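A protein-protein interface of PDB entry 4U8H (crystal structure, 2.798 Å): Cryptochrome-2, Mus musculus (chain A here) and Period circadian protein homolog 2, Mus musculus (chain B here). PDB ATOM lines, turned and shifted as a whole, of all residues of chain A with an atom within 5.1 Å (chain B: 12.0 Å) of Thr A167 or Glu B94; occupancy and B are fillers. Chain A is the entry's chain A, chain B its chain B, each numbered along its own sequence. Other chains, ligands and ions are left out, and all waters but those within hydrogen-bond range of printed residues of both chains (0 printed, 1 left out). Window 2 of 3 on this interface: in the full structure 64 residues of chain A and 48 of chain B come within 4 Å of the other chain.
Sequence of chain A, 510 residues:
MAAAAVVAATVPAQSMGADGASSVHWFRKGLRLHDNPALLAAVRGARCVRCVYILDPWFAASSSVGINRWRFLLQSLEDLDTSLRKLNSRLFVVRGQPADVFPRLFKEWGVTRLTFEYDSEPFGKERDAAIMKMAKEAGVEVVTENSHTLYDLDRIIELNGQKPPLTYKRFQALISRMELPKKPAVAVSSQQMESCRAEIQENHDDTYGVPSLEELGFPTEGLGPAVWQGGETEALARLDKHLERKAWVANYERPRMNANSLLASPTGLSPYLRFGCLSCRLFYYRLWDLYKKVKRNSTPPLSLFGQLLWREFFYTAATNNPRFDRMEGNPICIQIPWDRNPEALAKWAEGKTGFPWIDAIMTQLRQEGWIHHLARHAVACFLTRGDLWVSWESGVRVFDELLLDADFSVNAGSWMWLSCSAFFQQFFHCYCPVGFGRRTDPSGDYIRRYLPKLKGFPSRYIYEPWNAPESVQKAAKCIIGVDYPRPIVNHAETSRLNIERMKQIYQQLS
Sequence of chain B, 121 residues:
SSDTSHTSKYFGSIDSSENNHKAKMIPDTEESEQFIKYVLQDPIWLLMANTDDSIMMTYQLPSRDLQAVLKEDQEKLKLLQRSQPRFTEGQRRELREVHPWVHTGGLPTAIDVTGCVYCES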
ATOM      1  N   ASN A 160     -11.158 -37.910  10.399  1.00  0.00           N
ATOM      2  CA  ASN A 160     -12.102 -37.141  11.198  1.00  0.00           C
ATOM      3  C   ASN A 160     -13.498 -37.305  10.598  1.00  0.00           C
ATOM      4  O   ASN A 160     -14.379 -36.459  10.772  1.00  0.00           O
ATOM      5  CB  ASN A 160     -11.696 -35.651  11.261  1.00  0.00           C
ATOM      6  CG  ASN A 160     -12.335 -34.911  12.440  1.00  0.00           C
ATOM      7  OD1 ASN A 160     -12.296 -35.391  13.576  1.00  0.00           O
ATOM      8  ND2 ASN A 160     -12.928 -33.740  12.175  1.00  0.00           N
ATOM      9  N   PRO A 165     -11.499 -30.568  10.443  1.00  0.00           N
ATOM     10  CA  PRO A 165     -11.478 -30.119  11.835  1.00  0.00           C
ATOM     11  C   PRO A 165     -11.978 -28.698  11.944  1.00  0.00           C
ATOM     12  O   PRO A 165     -11.500 -27.846  11.208  1.00  0.00           O
ATOM     13  CB  PRO A 165      -9.998 -30.180  12.175  1.00  0.00           C
ATOM     14  CG  PRO A 165      -9.481 -31.315  11.337  1.00  0.00           C
ATOM     15  CD  PRO A 165     -10.288 -31.329  10.085  1.00  0.00           C
ATOM     16  N   LEU A 166     -12.915 -28.446  12.849  1.00  0.00           N
ATOM     17  CA  LEU A 166     -13.553 -27.136  12.966  1.00  0.00           C
ATOM     18  C   LEU A 166     -12.897 -26.252  14.010  1.00  0.00           C
ATOM     19  O   LEU A 166     -13.047 -25.031  13.978  1.00  0.00           O
ATOM     20  CB  LEU A 166     -15.040 -27.286  13.294  1.00  0.00           C
ATOM     21  CG  LEU A 166     -15.939 -27.946  12.248  1.00  0.00           C
ATOM     22  CD1 LEU A 166     -17.319 -28.118  12.849  1.00  0.00           C
ATOM     23  CD2 LEU A 166     -15.985 -27.122  10.944  1.00  0.00           C
ATOM     24  N   THR A 167     -12.189 -26.874  14.946  1.00  0.00           N
ATOM     25  CA  THR A 167     -11.422 -26.135  15.940  1.00  0.00           C
ATOM     26  C   THR A 167      -9.958 -26.508  15.845  1.00  0.00           C
ATOM     27  O   THR A 167      -9.613 -27.607  15.392  1.00  0.00           O
ATOM     28  CB  THR A 167     -11.881 -26.437  17.384  1.00  0.00           C
ATOM     29  OG1 THR A 167     -11.869 -27.853  17.610  1.00  0.00           O
ATOM     30  CG2 THR A 167     -13.272 -25.860  17.671  1.00  0.00           C
ATOM     31  N   TYR A 168      -9.103 -25.584  16.283  1.00  0.00           N
ATOM     32  CA  TYR A 168      -7.673 -25.836  16.380  1.00  0.00           C
ATOM     33  C   TYR A 168      -7.380 -26.952  17.391  1.00  0.00           C
ATOM     34  O   TYR A 168      -6.497 -27.779  17.138  1.00  0.00           O
ATOM     35  CB  TYR A 168      -6.925 -24.557  16.755  1.00  0.00           C
ATOM     36  CG  TYR A 168      -5.424 -24.701  16.688  1.00  0.00           C
ATOM     37  CD1 TYR A 168      -4.807 -25.321  15.598  1.00  0.00           C
ATOM     38  CD2 TYR A 168      -4.616 -24.219  17.701  1.00  0.00           C
ATOM     39  CE1 TYR A 168      -3.427 -25.457  15.529  1.00  0.00           C
ATOM     40  CE2 TYR A 168      -3.236 -24.359  17.641  1.00  0.00           C
ATOM     41  CZ  TYR A 168      -2.645 -24.967  16.552  1.00  0.00           C
ATOM     42  OH  TYR A 168      -1.268 -25.094  16.490  1.00  0.00           O
ATOM     43  N   LYS A 169      -8.111 -26.986  18.519  1.00  0.00           N
ATOM     44  CA  LYS A 169      -7.945 -28.084  19.496  1.00  0.00           C
ATOM     45  C   LYS A 169      -8.098 -29.474  18.874  1.00  0.00           C
ATOM     46  O   LYS A 169      -7.239 -30.338  19.085  1.00  0.00           O
ATOM     47  CB  LYS A 169      -8.837 -27.930  20.740  1.00  0.00           C
ATOM     48  CG  LYS A 169      -8.161 -27.169  21.882  1.00  0.00           C
ATOM     49  CD  LYS A 169      -9.147 -26.484  22.844  1.00  0.00           C
ATOM     50  CE  LYS A 169      -8.517 -25.216  23.454  1.00  0.00           C
ATOM     51  NZ  LYS A 169      -9.398 -24.524  24.437  1.00  0.00           N
ATOM     52  N   ARG A 170      -9.162 -29.671  18.091  1.00  0.00           N
ATOM     53  CA  ARG A 170      -9.374 -30.936  17.394  1.00  0.00           C
ATOM     54  C   ARG A 170      -8.352 -31.150  16.291  1.00  0.00           C
ATOM     55  O   ARG A 170      -7.967 -32.291  16.019  1.00  0.00           O
ATOM     56  CB  ARG A 170     -10.794 -31.033  16.816  1.00  0.00           C
ATOM     57  CG  ARG A 170     -11.099 -32.345  16.071  1.00  0.00           C
ATOM     58  CD  ARG A 170     -11.118 -33.575  16.995  1.00  0.00           C
ATOM     59  NE  ARG A 170     -12.167 -33.501  18.012  1.00  0.00           N
ATOM     60  CZ  ARG A 170     -12.142 -34.162  19.169  1.00  0.00           C
ATOM     61  NH1 ARG A 170     -11.115 -34.953  19.467  1.00  0.00           N
ATOM     62  NH2 ARG A 170     -13.141 -34.025  20.036  1.00  0.00           N
ATOM     63  N   PHE A 171      -7.923 -30.065  15.642  1.00  0.00           N
ATOM     64  CA  PHE A 171      -6.889 -30.181  14.616  1.00  0.00           C
ATOM     65  C   PHE A 171      -5.645 -30.787  15.248  1.00  0.00           C
ATOM     66  O   PHE A 171      -5.116 -31.801  14.768  1.00  0.00           O
ATOM     67  CB  PHE A 171      -6.534 -28.836  13.966  1.00  0.00           C
ATOM     68  CG  PHE A 171      -5.469 -28.969  12.919  1.00  0.00           C
ATOM     69  CD1 PHE A 171      -5.783 -29.460  11.650  1.00  0.00           C
ATOM     70  CD2 PHE A 171      -4.150 -28.672  13.214  1.00  0.00           C
ATOM     71  CE1 PHE A 171      -4.803 -29.640  10.691  1.00  0.00           C
ATOM     72  CE2 PHE A 171      -3.153 -28.859  12.257  1.00  0.00           C
ATOM     73  CZ  PHE A 171      -3.485 -29.345  10.994  1.00  0.00           C
ATOM     74  N   PHE A 313      -3.527 -26.047   9.652  1.00  0.00           N
ATOM     75  CA  PHE A 313      -4.941 -26.025  10.012  1.00  0.00           C
ATOM     76  C   PHE A 313      -5.743 -25.424   8.904  1.00  0.00           C
ATOM     77  O   PHE A 313      -6.668 -26.041   8.399  1.00  0.00           O
ATOM     78  CB  PHE A 313      -5.163 -25.173  11.254  1.00  0.00           C
ATOM     79  CG  PHE A 313      -6.618 -25.027  11.637  1.00  0.00           C
ATOM     80  CD1 PHE A 313      -7.403 -26.144  11.857  1.00  0.00           C
ATOM     81  CD2 PHE A 313      -7.190 -23.780  11.801  1.00  0.00           C
ATOM     82  CE1 PHE A 313      -8.732 -26.019  12.221  1.00  0.00           C
ATOM     83  CE2 PHE A 313      -8.521 -23.647  12.166  1.00  0.00           C
ATOM     84  CZ  PHE A 313      -9.291 -24.771  12.376  1.00  0.00           C
ATOM     85  N   PHE A 423     -15.076 -20.418  14.351  1.00  0.00           N
ATOM     86  CA  PHE A 423     -15.034 -21.079  15.646  1.00  0.00           C
ATOM     87  C   PHE A 423     -13.720 -21.815  15.842  1.00  0.00           C
ATOM     88  O   PHE A 423     -13.655 -22.829  16.542  1.00  0.00           O
ATOM     89  CB  PHE A 423     -16.225 -22.039  15.752  1.00  0.00           C
ATOM     90  CG  PHE A 423     -17.551 -21.341  15.859  1.00  0.00           C
ATOM     91  CD1 PHE A 423     -17.751 -20.357  16.812  1.00  0.00           C
ATOM     92  CD2 PHE A 423     -18.584 -21.641  14.990  1.00  0.00           C
ATOM     93  CE1 PHE A 423     -18.965 -19.692  16.915  1.00  0.00           C
ATOM     94  CE2 PHE A 423     -19.807 -20.977  15.085  1.00  0.00           C
ATOM     95  CZ  PHE A 423     -19.993 -20.002  16.055  1.00  0.00           C
ATOM     96  N   PHE A 424     -12.671 -21.301  15.217  1.00  0.00           N
ATOM     97  CA  PHE A 424     -11.373 -21.940  15.301  1.00  0.00           C
ATOM     98  C   PHE A 424     -10.810 -21.829  16.724  1.00  0.00           C
ATOM     99  O   PHE A 424     -10.053 -22.693  17.171  1.00  0.00           O
ATOM    100  CB  PHE A 424     -10.410 -21.337  14.272  1.00  0.00           C
ATOM    101  CG  PHE A 424     -10.991 -21.225  12.886  1.00  0.00           C
ATOM    102  CD1 PHE A 424     -11.580 -22.321  12.273  1.00  0.00           C
ATOM    103  CD2 PHE A 424     -10.974 -20.012  12.202  1.00  0.00           C
ATOM    104  CE1 PHE A 424     -12.134 -22.213  10.990  1.00  0.00           C
ATOM    105  CE2 PHE A 424     -11.525 -19.906  10.923  1.00  0.00           C
ATOM    106  CZ  PHE A 424     -12.115 -21.009  10.322  1.00  0.00           C
ATOM    107  N   ARG B  86     -24.967 -24.613  10.264  1.00  0.00           N
ATOM    108  CA  ARG B  86     -25.575 -25.678  11.041  1.00  0.00           C
ATOM    109  C   ARG B  86     -24.615 -26.860  11.084  1.00  0.00           C
ATOM    110  O   ARG B  86     -24.046 -27.261  10.068  1.00  0.00           O
ATOM    111  CB  ARG B  86     -26.927 -26.074  10.442  1.00  0.00           C
ATOM    112  CG  ARG B  86     -27.942 -24.931  10.468  1.00  0.00           C
ATOM    113  CD  ARG B  86     -29.320 -25.346   9.973  1.00  0.00           C
ATOM    114  NE  ARG B  86     -30.245 -24.214   9.964  1.00  0.00           N
ATOM    115  CZ  ARG B  86     -31.556 -24.325   9.778  1.00  0.00           C
ATOM    116  NH1 ARG B  86     -32.094 -25.524   9.589  1.00  0.00           N
ATOM    117  NH2 ARG B  86     -32.326 -23.244   9.788  1.00  0.00           N
ATOM    118  N   PHE B  87     -24.408 -27.387  12.282  1.00  0.00           N
ATOM    119  CA  PHE B  87     -23.533 -28.537  12.481  1.00  0.00           C
ATOM    120  C   PHE B  87     -24.366 -29.771  12.854  1.00  0.00           C
ATOM    121  O   PHE B  87     -25.598 -29.741  12.793  1.00  0.00           O
ATOM    122  CB  PHE B  87     -22.503 -28.245  13.583  1.00  0.00           C
ATOM    123  CG  PHE B  87     -21.980 -26.824  13.579  1.00  0.00           C
ATOM    124  CD1 PHE B  87     -21.052 -26.415  12.630  1.00  0.00           C
ATOM    125  CD2 PHE B  87     -22.407 -25.902  14.536  1.00  0.00           C
ATOM    126  CE1 PHE B  87     -20.574 -25.121  12.627  1.00  0.00           C
ATOM    127  CE2 PHE B  87     -21.928 -24.597  14.535  1.00  0.00           C
ATOM    128  CZ  PHE B  87     -21.009 -24.210  13.583  1.00  0.00           C
ATOM    129  N   THR B  88     -23.693 -30.852  13.234  1.00  0.00           N
ATOM    130  CA  THR B  88     -24.370 -32.057  13.704  1.00  0.00           C
ATOM    131  C   THR B  88     -23.706 -32.495  15.014  1.00  0.00           C
ATOM    132  O   THR B  88     -22.758 -31.866  15.449  1.00  0.00           O
ATOM    133  CB  THR B  88     -24.332 -33.185  12.639  1.00  0.00           C
ATOM    134  OG1 THR B  88     -24.333 -32.606  11.328  1.00  0.00           O
ATOM    135  CG2 THR B  88     -25.549 -34.121  12.775  1.00  0.00           C
ATOM    136  N   GLU B  89     -24.215 -33.550  15.643  1.00  0.00           N
ATOM    137  CA  GLU B  89     -23.730 -34.002  16.950  1.00  0.00           C
ATOM    138  C   GLU B  89     -22.206 -34.151  16.978  1.00  0.00           C
ATOM    139  O   GLU B  89     -21.548 -33.696  17.916  1.00  0.00           O
ATOM    140  CB  GLU B  89     -24.421 -35.315  17.351  1.00  0.00           C
ATOM    141  CG  GLU B  89     -25.945 -35.241  17.309  1.00  0.00           C
ATOM    142  CD  GLU B  89     -26.611 -36.607  17.293  1.00  0.00           C
ATOM    143  OE1 GLU B  89     -25.988 -37.569  16.796  1.00  0.00           O
ATOM    144  OE2 GLU B  89     -27.760 -36.722  17.775  1.00  0.00           O
ATOM    145  N   GLY B  90     -21.651 -34.753  15.928  1.00  0.00           N
ATOM    146  CA  GLY B  90     -20.215 -34.955  15.821  1.00  0.00           C
ATOM    147  C   GLY B  90     -19.400 -33.672  15.869  1.00  0.00           C
ATOM    148  O   GLY B  90     -18.289 -33.641  16.396  1.00  0.00           O
ATOM    149  N   GLN B  91     -19.965 -32.606  15.317  1.00  0.00           N
ATOM    150  CA  GLN B  91     -19.305 -31.306  15.267  1.00  0.00           C
ATOM    151  C   GLN B  91     -19.728 -30.407  16.431  1.00  0.00           C
ATOM    152  O   GLN B  91     -18.900 -29.730  17.037  1.00  0.00           O
ATOM    153  CB  GLN B  91     -19.616 -30.622  13.930  1.00  0.00           C
ATOM    154  CG  GLN B  91     -19.232 -31.455  12.706  1.00  0.00           C
ATOM    155  CD  GLN B  91     -19.803 -30.905  11.415  1.00  0.00           C
ATOM    156  OE1 GLN B  91     -20.709 -30.071  11.433  1.00  0.00           O
ATOM    157  NE2 GLN B  91     -19.281 -31.374  10.285  1.00  0.00           N
ATOM    158  N   ARG B  92     -21.020 -30.417  16.746  1.00  0.00           N
ATOM    159  CA  ARG B  92     -21.599 -29.523  17.755  1.00  0.00           C
ATOM    160  C   ARG B  92     -20.952 -29.641  19.136  1.00  0.00           C
ATOM    161  O   ARG B  92     -21.065 -28.734  19.961  1.00  0.00           O
ATOM    162  CB  ARG B  92     -23.111 -29.764  17.879  1.00  0.00           C
ATOM    163  CG  ARG B  92     -23.944 -29.333  16.673  1.00  0.00           C
ATOM    164  CD  ARG B  92     -25.359 -29.885  16.754  1.00  0.00           C
ATOM    165  NE  ARG B  92     -26.037 -29.441  17.967  1.00  0.00           N
ATOM    166  CZ  ARG B  92     -27.218 -29.889  18.379  1.00  0.00           C
ATOM    167  NH1 ARG B  92     -27.868 -30.808  17.673  1.00  0.00           N
ATOM    168  NH2 ARG B  92     -27.751 -29.417  19.501  1.00  0.00           N
ATOM    169  N   ARG B  93     -20.275 -30.761  19.376  1.00  0.00           N
ATOM    170  CA  ARG B  93     -19.694 -31.065  20.686  1.00  0.00           C
ATOM    171  C   ARG B  93     -18.348 -30.369  20.907  1.00  0.00           C
ATOM    172  O   ARG B  93     -18.004 -29.986  22.029  1.00  0.00           O
ATOM    173  CB  ARG B  93     -19.528 -32.588  20.834  1.00  0.00           C
ATOM    174  CG  ARG B  93     -19.443 -33.115  22.273  1.00  0.00           C
ATOM    175  CD  ARG B  93     -19.655 -34.636  22.324  1.00  0.00           C
ATOM    176  NE  ARG B  93     -20.926 -35.031  21.715  1.00  0.00           N
ATOM    177  CZ  ARG B  93     -21.096 -36.098  20.933  1.00  0.00           C
ATOM    178  NH1 ARG B  93     -20.066 -36.893  20.662  1.00  0.00           N
ATOM    179  NH2 ARG B  93     -22.296 -36.366  20.419  1.00  0.00           N
ATOM    180  N   GLU B  94     -17.597 -30.205  19.823  1.00  0.00           N
ATOM    181  CA  GLU B  94     -16.249 -29.664  19.896  1.00  0.00           C
ATOM    182  C   GLU B  94     -16.232 -28.201  20.293  1.00  0.00           C
ATOM    183  O   GLU B  94     -15.243 -27.711  20.810  1.00  0.00           O
ATOM    184  CB  GLU B  94     -15.544 -29.836  18.560  1.00  0.00           C
ATOM    185  CG  GLU B  94     -15.589 -31.251  18.051  1.00  0.00           C
ATOM    186  CD  GLU B  94     -14.659 -31.476  16.880  1.00  0.00           C
ATOM    187  OE1 GLU B  94     -14.314 -30.488  16.180  1.00  0.00           O
ATOM    188  OE2 GLU B  94     -14.272 -32.650  16.671  1.00  0.00           O
ATOM    189  N   LEU B  95     -17.330 -27.500  20.044  1.00  0.00           N
ATOM    190  CA  LEU B  95     -17.400 -26.088  20.389  1.00  0.00           C
ATOM    191  C   LEU B  95     -17.459 -25.899  21.894  1.00  0.00           C
ATOM    192  O   LEU B  95     -16.986 -24.893  22.407  1.00  0.00           O
ATOM    193  CB  LEU B  95     -18.596 -25.411  19.716  1.00  0.00           C
ATOM    194  CG  LEU B  95     -18.671 -25.587  18.200  1.00  0.00           C
ATOM    195  CD1 LEU B  95     -19.850 -24.821  17.640  1.00  0.00           C
ATOM    196  CD2 LEU B  95     -17.365 -25.154  17.525  1.00  0.00           C
ATOM    197  N   ARG B  96     -18.035 -26.869  22.601  1.00  0.00           N
ATOM    198  CA  ARG B  96     -18.124 -26.776  24.057  1.00  0.00           C
ATOM    199  C   ARG B  96     -16.743 -26.887  24.705  1.00  0.00           C
ATOM    200  O   ARG B  96     -16.493 -26.276  25.754  1.00  0.00           O
ATOM    201  CB  ARG B  96     -19.093 -27.818  24.621  1.00  0.00           C
ATOM    202  CG  ARG B  96     -20.545 -27.530  24.286  1.00  0.00           C
ATOM    203  CD  ARG B  96     -21.476 -28.611  24.809  1.00  0.00           C
ATOM    204  NE  ARG B  96     -22.770 -28.564  24.135  1.00  0.00           N
ATOM    205  CZ  ARG B  96     -23.703 -29.505  24.242  1.00  0.00           C
ATOM    206  NH1 ARG B  96     -23.487 -30.569  25.003  1.00  0.00           N
ATOM    207  NH2 ARG B  96     -24.852 -29.382  23.588  1.00  0.00           N
ATOM    208  N   GLU B  97     -15.849 -27.647  24.063  1.00  0.00           N
ATOM    209  CA  GLU B  97     -14.454 -27.775  24.505  1.00  0.00           C
ATOM    210  C   GLU B  97     -13.628 -26.498  24.317  1.00  0.00           C
ATOM    211  O   GLU B  97     -12.660 -26.271  25.044  1.00  0.00           O
ATOM    212  CB  GLU B  97     -13.769 -28.932  23.787  1.00  0.00           C
ATOM    213  CG  GLU B  97     -14.632 -30.172  23.664  1.00  0.00           C
ATOM    214  CD  GLU B  97     -13.985 -31.245  22.815  1.00  0.00           C
ATOM    215  OE1 GLU B  97     -12.953 -30.949  22.176  1.00  0.00           O
ATOM    216  OE2 GLU B  97     -14.503 -32.381  22.777  1.00  0.00           O
ATOM    217  N   VAL B  98     -14.005 -25.667  23.348  1.00  0.00           N
ATOM    218  CA  VAL B  98     -13.276 -24.433  23.081  1.00  0.00           C
ATOM    219  C   VAL B  98     -14.104 -23.214  23.476  1.00  0.00           C
ATOM    220  O   VAL B  98     -13.570 -22.153  23.797  1.00  0.00           O
ATOM    221  CB  VAL B  98     -12.878 -24.335  21.595  1.00  0.00           C
ATOM    222  CG1 VAL B  98     -11.785 -23.296  21.405  1.00  0.00           C
ATOM    223  CG2 VAL B  98     -12.410 -25.687  21.083  1.00  0.00           C
ATOM    224  N   HIS B  99     -15.422 -23.372  23.452  1.00  0.00           N
ATOM    225  CA  HIS B  99     -16.313 -22.266  23.784  1.00  0.00           C
ATOM    226  C   HIS B  99     -17.239 -22.588  24.965  1.00  0.00           C
ATOM    227  O   HIS B  99     -17.722 -23.717  25.107  1.00  0.00           O
ATOM    228  CB  HIS B  99     -17.143 -21.866  22.557  1.00  0.00           C
ATOM    229  CG  HIS B  99     -16.316 -21.406  21.389  1.00  0.00           C
ATOM    230  ND1 HIS B  99     -15.823 -20.128  21.290  1.00  0.00           N
ATOM    231  CD2 HIS B  99     -15.901 -22.069  20.282  1.00  0.00           C
ATOM    232  CE1 HIS B  99     -15.134 -20.013  20.160  1.00  0.00           C
ATOM    233  NE2 HIS B  99     -15.162 -21.174  19.541  1.00  0.00           N
ATOM    234  N   PRO B 100     -17.445 -21.597  25.838  1.00  0.00           N
ATOM    235  CA  PRO B 100     -18.520 -21.515  26.830  1.00  0.00           C
ATOM    236  C   PRO B 100     -19.906 -21.842  26.241  1.00  0.00           C
ATOM    237  O   PRO B 100     -20.674 -20.936  25.867  1.00  0.00           O
ATOM    238  CB  PRO B 100     -18.458 -20.054  27.273  1.00  0.00           C
ATOM    239  CG  PRO B 100     -17.082 -19.556  26.841  1.00  0.00           C
ATOM    240  CD  PRO B 100     -16.365 -20.648  26.139  1.00  0.00           C
ATOM    241  N   TRP B 101     -20.184 -23.147  26.171  1.00  0.00           N
ATOM    242  CA  TRP B 101     -21.478 -23.741  25.786  1.00  0.00           C
ATOM    243  C   TRP B 101     -22.282 -22.967  24.727  1.00  0.00           C
ATOM    244  O   TRP B 101     -21.801 -22.730  23.614  1.00  0.00           O
ATOM    245  CB  TRP B 101     -22.322 -24.084  27.044  1.00  0.00           C
ATOM    246  CG  TRP B 101     -22.617 -22.915  27.959  1.00  0.00           C
ATOM    247  CD1 TRP B 101     -21.833 -22.452  28.979  1.00  0.00           C
ATOM    248  CD2 TRP B 101     -23.781 -22.068  27.934  1.00  0.00           C
ATOM    249  NE1 TRP B 101     -22.440 -21.381  29.594  1.00  0.00           N
ATOM    250  CE2 TRP B 101     -23.633 -21.127  28.972  1.00  0.00           C
ATOM    251  CE3 TRP B 101     -24.934 -22.023  27.142  1.00  0.00           C
ATOM    252  CZ2 TRP B 101     -24.594 -20.152  29.236  1.00  0.00           C
ATOM    253  CZ3 TRP B 101     -25.883 -21.054  27.403  1.00  0.00           C
ATOM    254  CH2 TRP B 101     -25.708 -20.133  28.441  1.00  0.00           C
ATOM    255  N   LEU B 107     -20.277 -18.458  25.202  1.00  0.00           N
ATOM    256  CA  LEU B 107     -19.927 -17.643  24.037  1.00  0.00           C
ATOM    257  C   LEU B 107     -20.010 -16.133  24.217  1.00  0.00           C
ATOM    258  O   LEU B 107     -19.199 -15.410  23.648  1.00  0.00           O
ATOM    259  CB  LEU B 107     -20.739 -18.068  22.808  1.00  0.00           C
ATOM    260  CG  LEU B 107     -19.965 -19.124  22.036  1.00  0.00           C
ATOM    261  CD1 LEU B 107     -20.392 -19.156  20.569  1.00  0.00           C
ATOM    262  CD2 LEU B 107     -18.488 -18.797  22.221  1.00  0.00           C
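OG1 of Thr A167 lies within hydrogen-bond range of N of Arg A170 (3.3 Å).
O of Pro B100 lies within hydrogen-bond range of N of Leu B107 (2.6 Å).
The guanidinium group (NE) of Arg A170 lies within salt-bridge range of the side-chain carboxylate (OE2) of Glu B94 (2.6 Å).
The side-chain carboxylate (OE2) of Glu B97 is in salt-bridge range of the guanidinium group (NH2) of Arg A170, 3.5 Å away.
Thr A167 touches two residues of chain B.
Glu B94 touches just these residues of chain A: Thr A167 and Arg A170.
No residue of chain B comes within 4 Å of Pro A165.
Of chain B, only Glu B97 (3.7 Å) and Val B98 (3.8 Å) come within 4 Å of Lys A169.
Arg A170 touches two residues of chain B.
Of the printed residues of chain A, Glu B97 touches Lys A169 (3.7 Å) and Arg A170 (3.5 Å).
Printed residues of chain A within 4 Å of Phe B87: Phe A423 (3.8 Å).
Of the printed residues of chain A, Leu B95 touches Phe A423 (3.8 Å).
The nearest residue of chain B that does not touch Thr A167 is Leu B95 (4.2 Å).
The nearest printed residue of chain A that does not touch Glu B97 is Thr A167 (5.6 Å).
Hydrophobic or aromatic side chains of chain B within 4 Å of the printed part of chain A: Phe B87, Leu B95, Val B98, His B99 and Leu B107.
Among the printed residues, Asp or Glu carboxylates within 4 Å of a Lys or Arg side-chain nitrogen of the other chain: Arg A170 with Glu B94 and Arg A170 with Glu B97.
Gln B91 touches Leu A166 (CB to CD1, 3.6 Å).
Glu B94 touches Thr A167.
Thr A167 touches Val B98.
O of Glu B97 touches NZ of Lys A169, at 3.7 Å.
Lys A169 touches Val B98.
Phe A423 touches Phe B87 (CE2 to CZ, 3.8 Å).
CB of Phe A423 touches CD2 of Leu B95 (3.8 Å).
His B99 touches Phe A423 (NE2 to O, 3.7 Å).
Phe A423 touches Leu B107 (CE1 to CD1, 3.96 Å).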
